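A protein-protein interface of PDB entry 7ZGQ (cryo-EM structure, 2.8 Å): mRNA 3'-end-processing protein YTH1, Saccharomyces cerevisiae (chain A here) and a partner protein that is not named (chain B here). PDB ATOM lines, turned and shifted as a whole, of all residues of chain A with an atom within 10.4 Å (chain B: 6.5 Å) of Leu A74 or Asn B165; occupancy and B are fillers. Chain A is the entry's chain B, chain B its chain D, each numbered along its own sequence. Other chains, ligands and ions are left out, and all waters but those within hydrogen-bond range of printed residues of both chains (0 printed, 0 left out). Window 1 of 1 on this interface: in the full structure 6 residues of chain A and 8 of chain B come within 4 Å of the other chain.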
ATOM      1  N   CYS A  67     -21.416  12.522  15.929  1.00  0.00           N
ATOM      2  CA  CYS A  67     -20.027  12.099  16.049  1.00  0.00           C
ATOM      3  C   CYS A  67     -19.967  10.711  16.674  1.00  0.00           C
ATOM      4  O   CYS A  67     -20.454  10.504  17.790  1.00  0.00           O
ATOM      5  CB  CYS A  67     -19.231  13.099  16.887  1.00  0.00           C
ATOM      6  SG  CYS A  67     -17.473  12.722  17.027  1.00  0.00           S
ATOM      7  N   ARG A  68     -19.368   9.762  15.951  1.00  0.00           N
ATOM      8  CA  ARG A  68     -19.181   8.424  16.500  1.00  0.00           C
ATOM      9  C   ARG A  68     -18.231   8.439  17.689  1.00  0.00           C
ATOM     10  O   ARG A  68     -18.395   7.645  18.622  1.00  0.00           O
ATOM     11  CB  ARG A  68     -18.665   7.478  15.417  1.00  0.00           C
ATOM     12  N   HIS A  69     -17.235   9.328  17.673  1.00  0.00           N
ATOM     13  CA  HIS A  69     -16.322   9.439  18.805  1.00  0.00           C
ATOM     14  C   HIS A  69     -17.014  10.031  20.025  1.00  0.00           C
ATOM     15  O   HIS A  69     -16.687   9.666  21.160  1.00  0.00           O
ATOM     16  CB  HIS A  69     -15.108  10.283  18.417  1.00  0.00           C
ATOM     17  CG  HIS A  69     -14.305   9.705  17.295  1.00  0.00           C
ATOM     18  ND1 HIS A  69     -13.363  10.433  16.601  1.00  0.00           N
ATOM     19  CD2 HIS A  69     -14.302   8.467  16.745  1.00  0.00           C
ATOM     20  CE1 HIS A  69     -12.815   9.670  15.673  1.00  0.00           C
ATOM     21  NE2 HIS A  69     -13.366   8.472  15.739  1.00  0.00           N
ATOM     22  N   TRP A  70     -17.961  10.947  19.815  1.00  0.00           N
ATOM     23  CA  TRP A  70     -18.712  11.505  20.935  1.00  0.00           C
ATOM     24  C   TRP A  70     -19.690  10.492  21.514  1.00  0.00           C
ATOM     25  O   TRP A  70     -19.949  10.505  22.722  1.00  0.00           O
ATOM     26  CB  TRP A  70     -19.451  12.768  20.493  1.00  0.00           C
ATOM     27  CG  TRP A  70     -20.204  13.448  21.592  1.00  0.00           C
ATOM     28  CD1 TRP A  70     -19.685  14.238  22.574  1.00  0.00           C
ATOM     29  CD2 TRP A  70     -21.617  13.405  21.816  1.00  0.00           C
ATOM     30  NE1 TRP A  70     -20.687  14.688  23.399  1.00  0.00           N
ATOM     31  CE2 TRP A  70     -21.882  14.190  22.954  1.00  0.00           C
ATOM     32  CE3 TRP A  70     -22.682  12.777  21.165  1.00  0.00           C
ATOM     33  CZ2 TRP A  70     -23.170  14.363  23.456  1.00  0.00           C
ATOM     34  CZ3 TRP A  70     -23.959  12.952  21.664  1.00  0.00           C
ATOM     35  CH2 TRP A  70     -24.191  13.738  22.799  1.00  0.00           C
ATOM     36  N   LEU A  71     -20.245   9.616  20.673  1.00  0.00           N
ATOM     37  CA  LEU A  71     -21.146   8.582  21.170  1.00  0.00           C
ATOM     38  C   LEU A  71     -20.423   7.629  22.112  1.00  0.00           C
ATOM     39  O   LEU A  71     -20.977   7.219  23.139  1.00  0.00           O
ATOM     40  CB  LEU A  71     -21.762   7.816  20.000  1.00  0.00           C
ATOM     41  CG  LEU A  71     -22.777   8.584  19.153  1.00  0.00           C
ATOM     42  CD1 LEU A  71     -23.228   7.745  17.968  1.00  0.00           C
ATOM     43  CD2 LEU A  71     -23.967   9.008  19.997  1.00  0.00           C
ATOM     44  N   ARG A  72     -19.186   7.266  21.781  1.00  0.00           N
ATOM     45  CA  ARG A  72     -18.377   6.403  22.631  1.00  0.00           C
ATOM     46  C   ARG A  72     -17.668   7.167  23.741  1.00  0.00           C
ATOM     47  O   ARG A  72     -16.965   6.547  24.545  1.00  0.00           O
ATOM     48  CB  ARG A  72     -17.347   5.650  21.785  1.00  0.00           C
ATOM     49  N   GLY A  73     -17.833   8.485  23.805  1.00  0.00           N
ATOM     50  CA  GLY A  73     -17.175   9.276  24.824  1.00  0.00           C
ATOM     51  C   GLY A  73     -15.700   9.497  24.600  1.00  0.00           C
ATOM     52  O   GLY A  73     -14.977   9.793  25.557  1.00  0.00           O
ATOM     53  N   LEU A  74     -15.226   9.367  23.363  1.00  0.00           N
ATOM     54  CA  LEU A  74     -13.808   9.471  23.036  1.00  0.00           C
ATOM     55  C   LEU A  74     -13.592  10.458  21.896  1.00  0.00           C
ATOM     56  O   LEU A  74     -12.854  10.199  20.945  1.00  0.00           O
ATOM     57  CB  LEU A  74     -13.236   8.104  22.680  1.00  0.00           C
ATOM     58  CG  LEU A  74     -13.269   7.072  23.806  1.00  0.00           C
ATOM     59  CD1 LEU A  74     -13.007   5.676  23.268  1.00  0.00           C
ATOM     60  CD2 LEU A  74     -12.266   7.441  24.887  1.00  0.00           C
ATOM     61  N   CYS A  75     -14.243  11.614  21.981  1.00  0.00           N
ATOM     62  CA  CYS A  75     -14.069  12.670  20.993  1.00  0.00           C
ATOM     63  C   CYS A  75     -12.954  13.601  21.454  1.00  0.00           C
ATOM     64  O   CYS A  75     -13.087  14.276  22.479  1.00  0.00           O
ATOM     65  CB  CYS A  75     -15.370  13.442  20.785  1.00  0.00           C
ATOM     66  SG  CYS A  75     -15.378  14.494  19.313  1.00  0.00           S
ATOM     67  N   LYS A  76     -11.854  13.629  20.697  1.00  0.00           N
ATOM     68  CA  LYS A  76     -10.725  14.479  21.060  1.00  0.00           C
ATOM     69  C   LYS A  76     -11.094  15.955  20.986  1.00  0.00           C
ATOM     70  O   LYS A  76     -10.701  16.743  21.853  1.00  0.00           O
ATOM     71  CB  LYS A  76      -9.531  14.176  20.156  1.00  0.00           C
ATOM     72  CG  LYS A  76      -9.422  12.717  19.741  1.00  0.00           C
ATOM     73  CD  LYS A  76      -8.392  11.977  20.579  1.00  0.00           C
ATOM     74  CE  LYS A  76      -8.504  10.472  20.391  1.00  0.00           C
ATOM     75  NZ  LYS A  76      -9.468   9.860  21.347  1.00  0.00           N
ATOM     76  N   LYS A  77     -11.847  16.346  19.962  1.00  0.00           N
ATOM     77  CA  LYS A  77     -12.266  17.733  19.804  1.00  0.00           C
ATOM     78  C   LYS A  77     -13.530  17.977  20.619  1.00  0.00           C
ATOM     79  O   LYS A  77     -14.585  17.405  20.325  1.00  0.00           O
ATOM     80  CB  LYS A  77     -12.496  18.050  18.329  1.00  0.00           C
ATOM     81  CG  LYS A  77     -11.647  17.214  17.382  1.00  0.00           C
ATOM     82  CD  LYS A  77     -11.840  17.634  15.935  1.00  0.00           C
ATOM     83  CE  LYS A  77     -12.745  16.664  15.193  1.00  0.00           C
ATOM     84  NZ  LYS A  77     -12.160  15.297  15.134  1.00  0.00           N
ATOM     85  N   ASN A  78     -13.420  18.818  21.648  1.00  0.00           N
ATOM     86  CA  ASN A  78     -14.540  19.101  22.536  1.00  0.00           C
ATOM     87  C   ASN A  78     -15.685  19.773  21.789  1.00  0.00           C
ATOM     88  O   ASN A  78     -16.772  19.199  21.659  1.00  0.00           O
ATOM     89  CB  ASN A  78     -14.084  19.982  23.701  1.00  0.00           C
ATOM     90  CG  ASN A  78     -12.639  19.734  24.087  1.00  0.00           C
ATOM     91  OD1 ASN A  78     -11.722  20.316  23.507  1.00  0.00           O
ATOM     92  ND2 ASN A  78     -12.429  18.869  25.072  1.00  0.00           N
ATOM     93  N   ASP A  79     -15.448  20.985  21.287  1.00  0.00           N
ATOM     94  CA  ASP A  79     -16.459  21.739  20.563  1.00  0.00           C
ATOM     95  C   ASP A  79     -16.041  22.116  19.151  1.00  0.00           C
ATOM     96  O   ASP A  79     -16.871  22.642  18.400  1.00  0.00           O
ATOM     97  CB  ASP A  79     -16.828  23.018  21.333  1.00  0.00           C
ATOM     98  N   GLN A  80     -14.791  21.868  18.768  1.00  0.00           N
ATOM     99  CA  GLN A  80     -14.320  22.144  17.419  1.00  0.00           C
ATOM    100  C   GLN A  80     -14.632  21.017  16.444  1.00  0.00           C
ATOM    101  O   GLN A  80     -14.292  21.132  15.262  1.00  0.00           O
ATOM    102  CB  GLN A  80     -12.812  22.408  17.433  1.00  0.00           C
ATOM    103  CG  GLN A  80     -12.415  23.726  18.081  1.00  0.00           C
ATOM    104  CD  GLN A  80     -12.268  23.619  19.586  1.00  0.00           C
ATOM    105  OE1 GLN A  80     -13.151  23.110  20.274  1.00  0.00           O
ATOM    106  NE2 GLN A  80     -11.146  24.104  20.106  1.00  0.00           N
ATOM    107  N   CYS A  81     -15.257  19.939  16.911  1.00  0.00           N
ATOM    108  CA  CYS A  81     -15.578  18.820  16.038  1.00  0.00           C
ATOM    109  C   CYS A  81     -16.562  19.245  14.956  1.00  0.00           C
ATOM    110  O   CYS A  81     -17.503  20.002  15.208  1.00  0.00           O
ATOM    111  CB  CYS A  81     -16.158  17.664  16.852  1.00  0.00           C
ATOM    112  SG  CYS A  81     -16.744  16.273  15.862  1.00  0.00           S
ATOM    113  N   HIS A  85     -22.546  16.957  18.078  1.00  0.00           N
ATOM    114  CA  HIS A  85     -22.478  16.380  19.420  1.00  0.00           C
ATOM    115  C   HIS A  85     -23.862  16.428  20.066  1.00  0.00           C
ATOM    116  O   HIS A  85     -24.120  17.152  21.028  1.00  0.00           O
ATOM    117  CB  HIS A  85     -21.434  17.112  20.259  1.00  0.00           C
ATOM    118  CG  HIS A  85     -20.022  16.753  19.914  1.00  0.00           C
ATOM    119  ND1 HIS A  85     -18.939  17.244  20.608  1.00  0.00           N
ATOM    120  CD2 HIS A  85     -19.518  15.950  18.948  1.00  0.00           C
ATOM    121  CE1 HIS A  85     -17.827  16.760  20.084  1.00  0.00           C
ATOM    122  NE2 HIS A  85     -18.150  15.972  19.075  1.00  0.00           N
ATOM    123  N   ARG B 107     -13.261   1.192  31.050  1.00  0.00           N
ATOM    124  CA  ARG B 107     -12.278   0.741  30.078  1.00  0.00           C
ATOM    125  C   ARG B 107     -10.923   0.587  30.750  1.00  0.00           C
ATOM    126  O   ARG B 107     -10.627   1.249  31.748  1.00  0.00           O
ATOM    127  CB  ARG B 107     -12.162   1.714  28.898  1.00  0.00           C
ATOM    128  CG  ARG B 107     -13.422   1.830  28.063  1.00  0.00           C
ATOM    129  CD  ARG B 107     -13.196   2.707  26.849  1.00  0.00           C
ATOM    130  NE  ARG B 107     -14.401   2.829  26.039  1.00  0.00           N
ATOM    131  CZ  ARG B 107     -15.100   3.948  25.900  1.00  0.00           C
ATOM    132  NH1 ARG B 107     -14.739   5.067  26.508  1.00  0.00           N
ATOM    133  NH2 ARG B 107     -16.184   3.944  25.132  1.00  0.00           N
ATOM    134  N   LEU B 119      -7.241   1.189  24.425  1.00  0.00           N
ATOM    135  CA  LEU B 119      -8.390   1.065  25.307  1.00  0.00           C
ATOM    136  C   LEU B 119      -9.061  -0.289  25.122  1.00  0.00           C
ATOM    137  O   LEU B 119      -9.020  -0.882  24.042  1.00  0.00           O
ATOM    138  CB  LEU B 119      -9.393   2.187  25.046  1.00  0.00           C
ATOM    139  CG  LEU B 119      -8.817   3.602  25.066  1.00  0.00           C
ATOM    140  CD1 LEU B 119      -9.930   4.624  24.980  1.00  0.00           C
ATOM    141  CD2 LEU B 119      -7.980   3.823  26.315  1.00  0.00           C
ATOM    142  N   ASN B 121     -12.732  -2.299  26.503  1.00  0.00           N
ATOM    143  CA  ASN B 121     -13.978  -2.204  27.254  1.00  0.00           C
ATOM    144  C   ASN B 121     -14.039  -3.283  28.328  1.00  0.00           C
ATOM    145  O   ASN B 121     -13.690  -4.442  28.083  1.00  0.00           O
ATOM    146  CB  ASN B 121     -15.177  -2.325  26.316  1.00  0.00           C
ATOM    147  CG  ASN B 121     -15.145  -1.304  25.200  1.00  0.00           C
ATOM    148  OD1 ASN B 121     -14.797  -0.142  25.415  1.00  0.00           O
ATOM    149  ND2 ASN B 121     -15.518  -1.730  24.000  1.00  0.00           N
ATOM    150  N   PHE B 127     -11.423  -4.385  22.136  1.00  0.00           N
ATOM    151  CA  PHE B 127     -11.285  -3.109  21.442  1.00  0.00           C
ATOM    152  C   PHE B 127      -9.907  -3.070  20.801  1.00  0.00           C
ATOM    153  O   PHE B 127      -9.006  -3.820  21.184  1.00  0.00           O
ATOM    154  CB  PHE B 127     -11.461  -1.907  22.376  1.00  0.00           C
ATOM    155  CG  PHE B 127     -12.343  -0.830  21.811  1.00  0.00           C
ATOM    156  CD1 PHE B 127     -12.326  -0.536  20.460  1.00  0.00           C
ATOM    157  CD2 PHE B 127     -13.178  -0.100  22.639  1.00  0.00           C
ATOM    158  CE1 PHE B 127     -13.145   0.451  19.940  1.00  0.00           C
ATOM    159  CE2 PHE B 127     -13.994   0.893  22.129  1.00  0.00           C
ATOM    160  CZ  PHE B 127     -13.975   1.171  20.778  1.00  0.00           C
ATOM    161  N   THR B 129      -8.518   0.342  19.916  1.00  0.00           N
ATOM    162  CA  THR B 129      -8.398   1.795  19.780  1.00  0.00           C
ATOM    163  C   THR B 129      -6.969   2.221  20.094  1.00  0.00           C
ATOM    164  O   THR B 129      -6.617   2.556  21.226  1.00  0.00           O
ATOM    165  CB  THR B 129      -9.391   2.512  20.687  1.00  0.00           C
ATOM    166  OG1 THR B 129     -10.703   1.990  20.471  1.00  0.00           O
ATOM    167  CG2 THR B 129      -9.401   4.004  20.393  1.00  0.00           C
ATOM    168  N   MET B 131      -4.214   5.063  19.955  1.00  0.00           N
ATOM    169  CA  MET B 131      -4.379   6.497  20.140  1.00  0.00           C
ATOM    170  C   MET B 131      -3.124   7.315  19.880  1.00  0.00           C
ATOM    171  O   MET B 131      -3.248   8.525  19.651  1.00  0.00           O
ATOM    172  CB  MET B 131      -4.876   6.796  21.562  1.00  0.00           C
ATOM    173  CG  MET B 131      -5.667   8.084  21.688  1.00  0.00           C
ATOM    174  SD  MET B 131      -6.954   7.968  22.940  1.00  0.00           S
ATOM    175  CE  MET B 131      -7.539   6.299  22.663  1.00  0.00           C
ATOM    176  N   TRP B 162      -4.277  14.499  30.787  1.00  0.00           N
ATOM    177  CA  TRP B 162      -5.339  14.126  29.868  1.00  0.00           C
ATOM    178  C   TRP B 162      -6.706  14.426  30.466  1.00  0.00           C
ATOM    179  O   TRP B 162      -6.853  14.706  31.658  1.00  0.00           O
ATOM    180  CB  TRP B 162      -5.249  12.640  29.501  1.00  0.00           C
ATOM    181  CG  TRP B 162      -3.938  12.249  28.912  1.00  0.00           C
ATOM    182  CD1 TRP B 162      -2.784  11.985  29.584  1.00  0.00           C
ATOM    183  CD2 TRP B 162      -3.647  12.068  27.524  1.00  0.00           C
ATOM    184  NE1 TRP B 162      -1.787  11.656  28.701  1.00  0.00           N
ATOM    185  CE2 TRP B 162      -2.291  11.699  27.428  1.00  0.00           C
ATOM    186  CE3 TRP B 162      -4.398  12.184  26.352  1.00  0.00           C
ATOM    187  CZ2 TRP B 162      -1.674  11.444  26.208  1.00  0.00           C
ATOM    188  CZ3 TRP B 162      -3.785  11.928  25.144  1.00  0.00           C
ATOM    189  CH2 TRP B 162      -2.436  11.564  25.080  1.00  0.00           C
ATOM    190  N   GLN B 163      -7.707  14.360  29.603  1.00  0.00           N
ATOM    191  CA  GLN B 163      -9.114  14.455  29.936  1.00  0.00           C
ATOM    192  C   GLN B 163      -9.762  13.082  29.810  1.00  0.00           C
ATOM    193  O   GLN B 163      -9.219  12.191  29.148  1.00  0.00           O
ATOM    194  CB  GLN B 163      -9.817  15.453  29.007  1.00  0.00           C
ATOM    195  CG  GLN B 163     -10.240  16.745  29.681  1.00  0.00           C
ATOM    196  CD  GLN B 163     -10.968  17.680  28.736  1.00  0.00           C
ATOM    197  OE1 GLN B 163     -11.089  17.405  27.544  1.00  0.00           O
ATOM    198  NE2 GLN B 163     -11.457  18.794  29.266  1.00  0.00           N
ATOM    199  N   PRO B 164     -10.913  12.862  30.451  1.00  0.00           N
ATOM    200  CA  PRO B 164     -11.558  11.542  30.341  1.00  0.00           C
ATOM    201  C   PRO B 164     -11.888  11.147  28.912  1.00  0.00           C
ATOM    202  O   PRO B 164     -11.941   9.947  28.611  1.00  0.00           O
ATOM    203  CB  PRO B 164     -12.825  11.693  31.197  1.00  0.00           C
ATOM    204  CG  PRO B 164     -12.990  13.165  31.419  1.00  0.00           C
ATOM    205  CD  PRO B 164     -11.617  13.739  31.400  1.00  0.00           C
ATOM    206  N   ASN B 165     -12.109  12.111  28.021  1.00  0.00           N
ATOM    207  CA  ASN B 165     -12.301  11.831  26.606  1.00  0.00           C
ATOM    208  C   ASN B 165     -10.982  11.749  25.844  1.00  0.00           C
ATOM    209  O   ASN B 165     -10.996  11.692  24.611  1.00  0.00           O
ATOM    210  CB  ASN B 165     -13.216  12.883  25.971  1.00  0.00           C
ATOM    211  CG  ASN B 165     -12.568  14.252  25.883  1.00  0.00           C
ATOM    212  OD1 ASN B 165     -11.597  14.540  26.580  1.00  0.00           O
ATOM    213  ND2 ASN B 165     -13.106  15.104  25.020  1.00  0.00           N
ATOM    214  N   PHE B 166      -9.852  11.759  26.556  1.00  0.00           N
ATOM    215  CA  PHE B 166      -8.522  11.567  25.971  1.00  0.00           C
ATOM    216  C   PHE B 166      -8.158  12.699  25.011  1.00  0.00           C
ATOM    217  O   PHE B 166      -7.816  12.472  23.851  1.00  0.00           O
ATOM    218  CB  PHE B 166      -8.413  10.204  25.286  1.00  0.00           C
ATOM    219  CG  PHE B 166      -8.176   9.074  26.239  1.00  0.00           C
ATOM    220  CD1 PHE B 166      -6.955   8.934  26.875  1.00  0.00           C
ATOM    221  CD2 PHE B 166      -9.177   8.160  26.513  1.00  0.00           C
ATOM    222  CE1 PHE B 166      -6.735   7.899  27.758  1.00  0.00           C
ATOM    223  CE2 PHE B 166      -8.962   7.122  27.397  1.00  0.00           C
ATOM    224  CZ  PHE B 166      -7.740   6.991  28.020  1.00  0.00           C
ATOM    225  N   SER B 167      -8.232  13.928  25.511  1.00  0.00           N
ATOM    226  CA  SER B 167      -7.798  15.109  24.782  1.00  0.00           C
ATOM    227  C   SER B 167      -6.672  15.794  25.544  1.00  0.00           C
ATOM    228  O   SER B 167      -6.592  15.708  26.773  1.00  0.00           O
ATOM    229  CB  SER B 167      -8.954  16.092  24.566  1.00  0.00           C
ATOM    230  OG  SER B 167     -10.160  15.407  24.285  1.00  0.00           O
ATOM    231  N   MET B 168      -5.795  16.464  24.800  1.00  0.00           N
ATOM    232  CA  MET B 168      -4.710  17.216  25.415  1.00  0.00           C
ATOM    233  C   MET B 168      -5.247  18.301  26.337  1.00  0.00           C
ATOM    234  O   MET B 168      -6.092  19.113  25.948  1.00  0.00           O
ATOM    235  CB  MET B 168      -3.823  17.853  24.340  1.00  0.00           C
ATOM    236  CG  MET B 168      -2.303  17.811  24.587  1.00  0.00           C
ATOM    237  SD  MET B 168      -1.505  16.347  25.294  1.00  0.00           S
ATOM    238  CE  MET B 168      -2.366  14.991  24.503  1.00  0.00           C
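Leu A74 touches just these residues of chain B: Arg B107 (3.7 Å), Leu B119 (3.7 Å), Asn B165 (3.9 Å) and Phe B166 (3.6 Å).
Asn B165 touches four residues of chain A.
Gln B163 touches one residue of chain A.
No residue of chain A comes within 4 Å of Pro B164.
Of chain A, only Leu A74 (3.6 Å) and Lys A76 (3.4 Å) come within 4 Å of Phe B166.
Printed residues of chain A within 4 Å of Met B131: Lys A76 (3.5 Å).
Printed residues of chain B within 4 Å of Gly A73: Asn B165.
Of the printed residues of chain B, Asn A78 touches Gln B163 and Asn B165.
Of the printed residues of chain A, Leu B119 touches Leu A74 (3.7 Å).
Of the printed residues of chain A, Arg B107 touches Arg A72 (2.8 Å) and Leu A74 (3.7 Å).
The nearest residue of chain A that does not touch Asn B165 is Lys A76 (4.04 Å).
The nearest printed residue of chain B that does not touch Arg A72 is Phe B127 (5.7 Å).
The side-chain sulfur of Cys A75 sits at hydrogen-bond distance from the side-chain sulfur of Cys A67 (3.6 Å).
The backbone carbonyl oxygen (O) of His A69 lies within hydrogen-bond range of the backbone NH (N) of Leu A74 (2.7 Å).
O of Lys A77 is in hydrogen-bond range of SG of Cys A75 (3.2 Å).
NE2 of His A85 is in hydrogen-bond range of SG of Cys A75, 3.2 Å away.
O of Asn A78 lies close to ND1 of His A85 (3.1 Å).
The guanidinium group of Arg B107 lies within hydrogen-bond range of the side-chain amide oxygen of Asn B121 (3.1 Å).
The backbone carbonyl oxygen (O) of Arg A72 sits at hydrogen-bond distance from the guanidinium group (NH2) of Arg B107 (2.8 Å).
The backbone carbonyl oxygen of Cys A75 is in hydrogen-bond range of the side-chain amide nitrogen of Asn B165, at 2.7 Å.
SD of Met B131 lies within hydrogen-bond range of NZ of Lys A76, at 3.5 Å.
The backbone carbonyl oxygen of Lys A76 sits at hydrogen-bond distance from the side-chain hydroxyl of Ser B167 (2.8 Å).
OE1 of Gln B163 lies within hydrogen-bond range of ND2 of Asn A78, at 3.2 Å.
Gly A73 touches Asn B165.
CG of Leu A74 touches NH1 of Arg B107, 3.7 Å away.
Leu A74 touches Leu B119.
Leu A74 touches Asn B165 (CA to O, 3.9 Å).
Leu A74 touches Phe B166.
O of Cys A75 touches OG of Ser B167 (3.6 Å).
Phe B166 touches Lys A76 (O to CD, 3.4 Å).
Asn A78 touches Asn B165 (ND2 to ND2, 3.8 Å).
Of the 13 printed residues of chain B, 7 touch a printed residue of chain A.
Printed residues of chain B that touch a printed residue of chain A: Arg B107, Leu B119, Met B131, Gln B163, Asn B165, Phe B166 and Ser B167.
Hydrophobic or aromatic side chains of chain B within 4 Å of the printed part of chain A: Leu B119, Met B131 and Phe B166.
Along chain B the printed residues that touch a printed residue of chain A span positions 107 to 167.
Of the 16 printed residues of chain A, 6 touch a printed residue of chain B.
Printed residues of chain A that touch a printed residue of chain B: Arg A72, Gly A73, Leu A74, Cys A75, Lys A76 and Asn A78.
Hydrophobic or aromatic side chains of chain A that line the printed part of chain B: Leu A74.
Along chain A the printed residues that touch a printed residue of chain B span positions 72 to 78.
Among the printed residues, 13 pairs touch across the chains.
Among the printed residues, no Asp or Glu carboxylate lies within 4 Å of a Lys or Arg side-chain nitrogen of the other chain.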
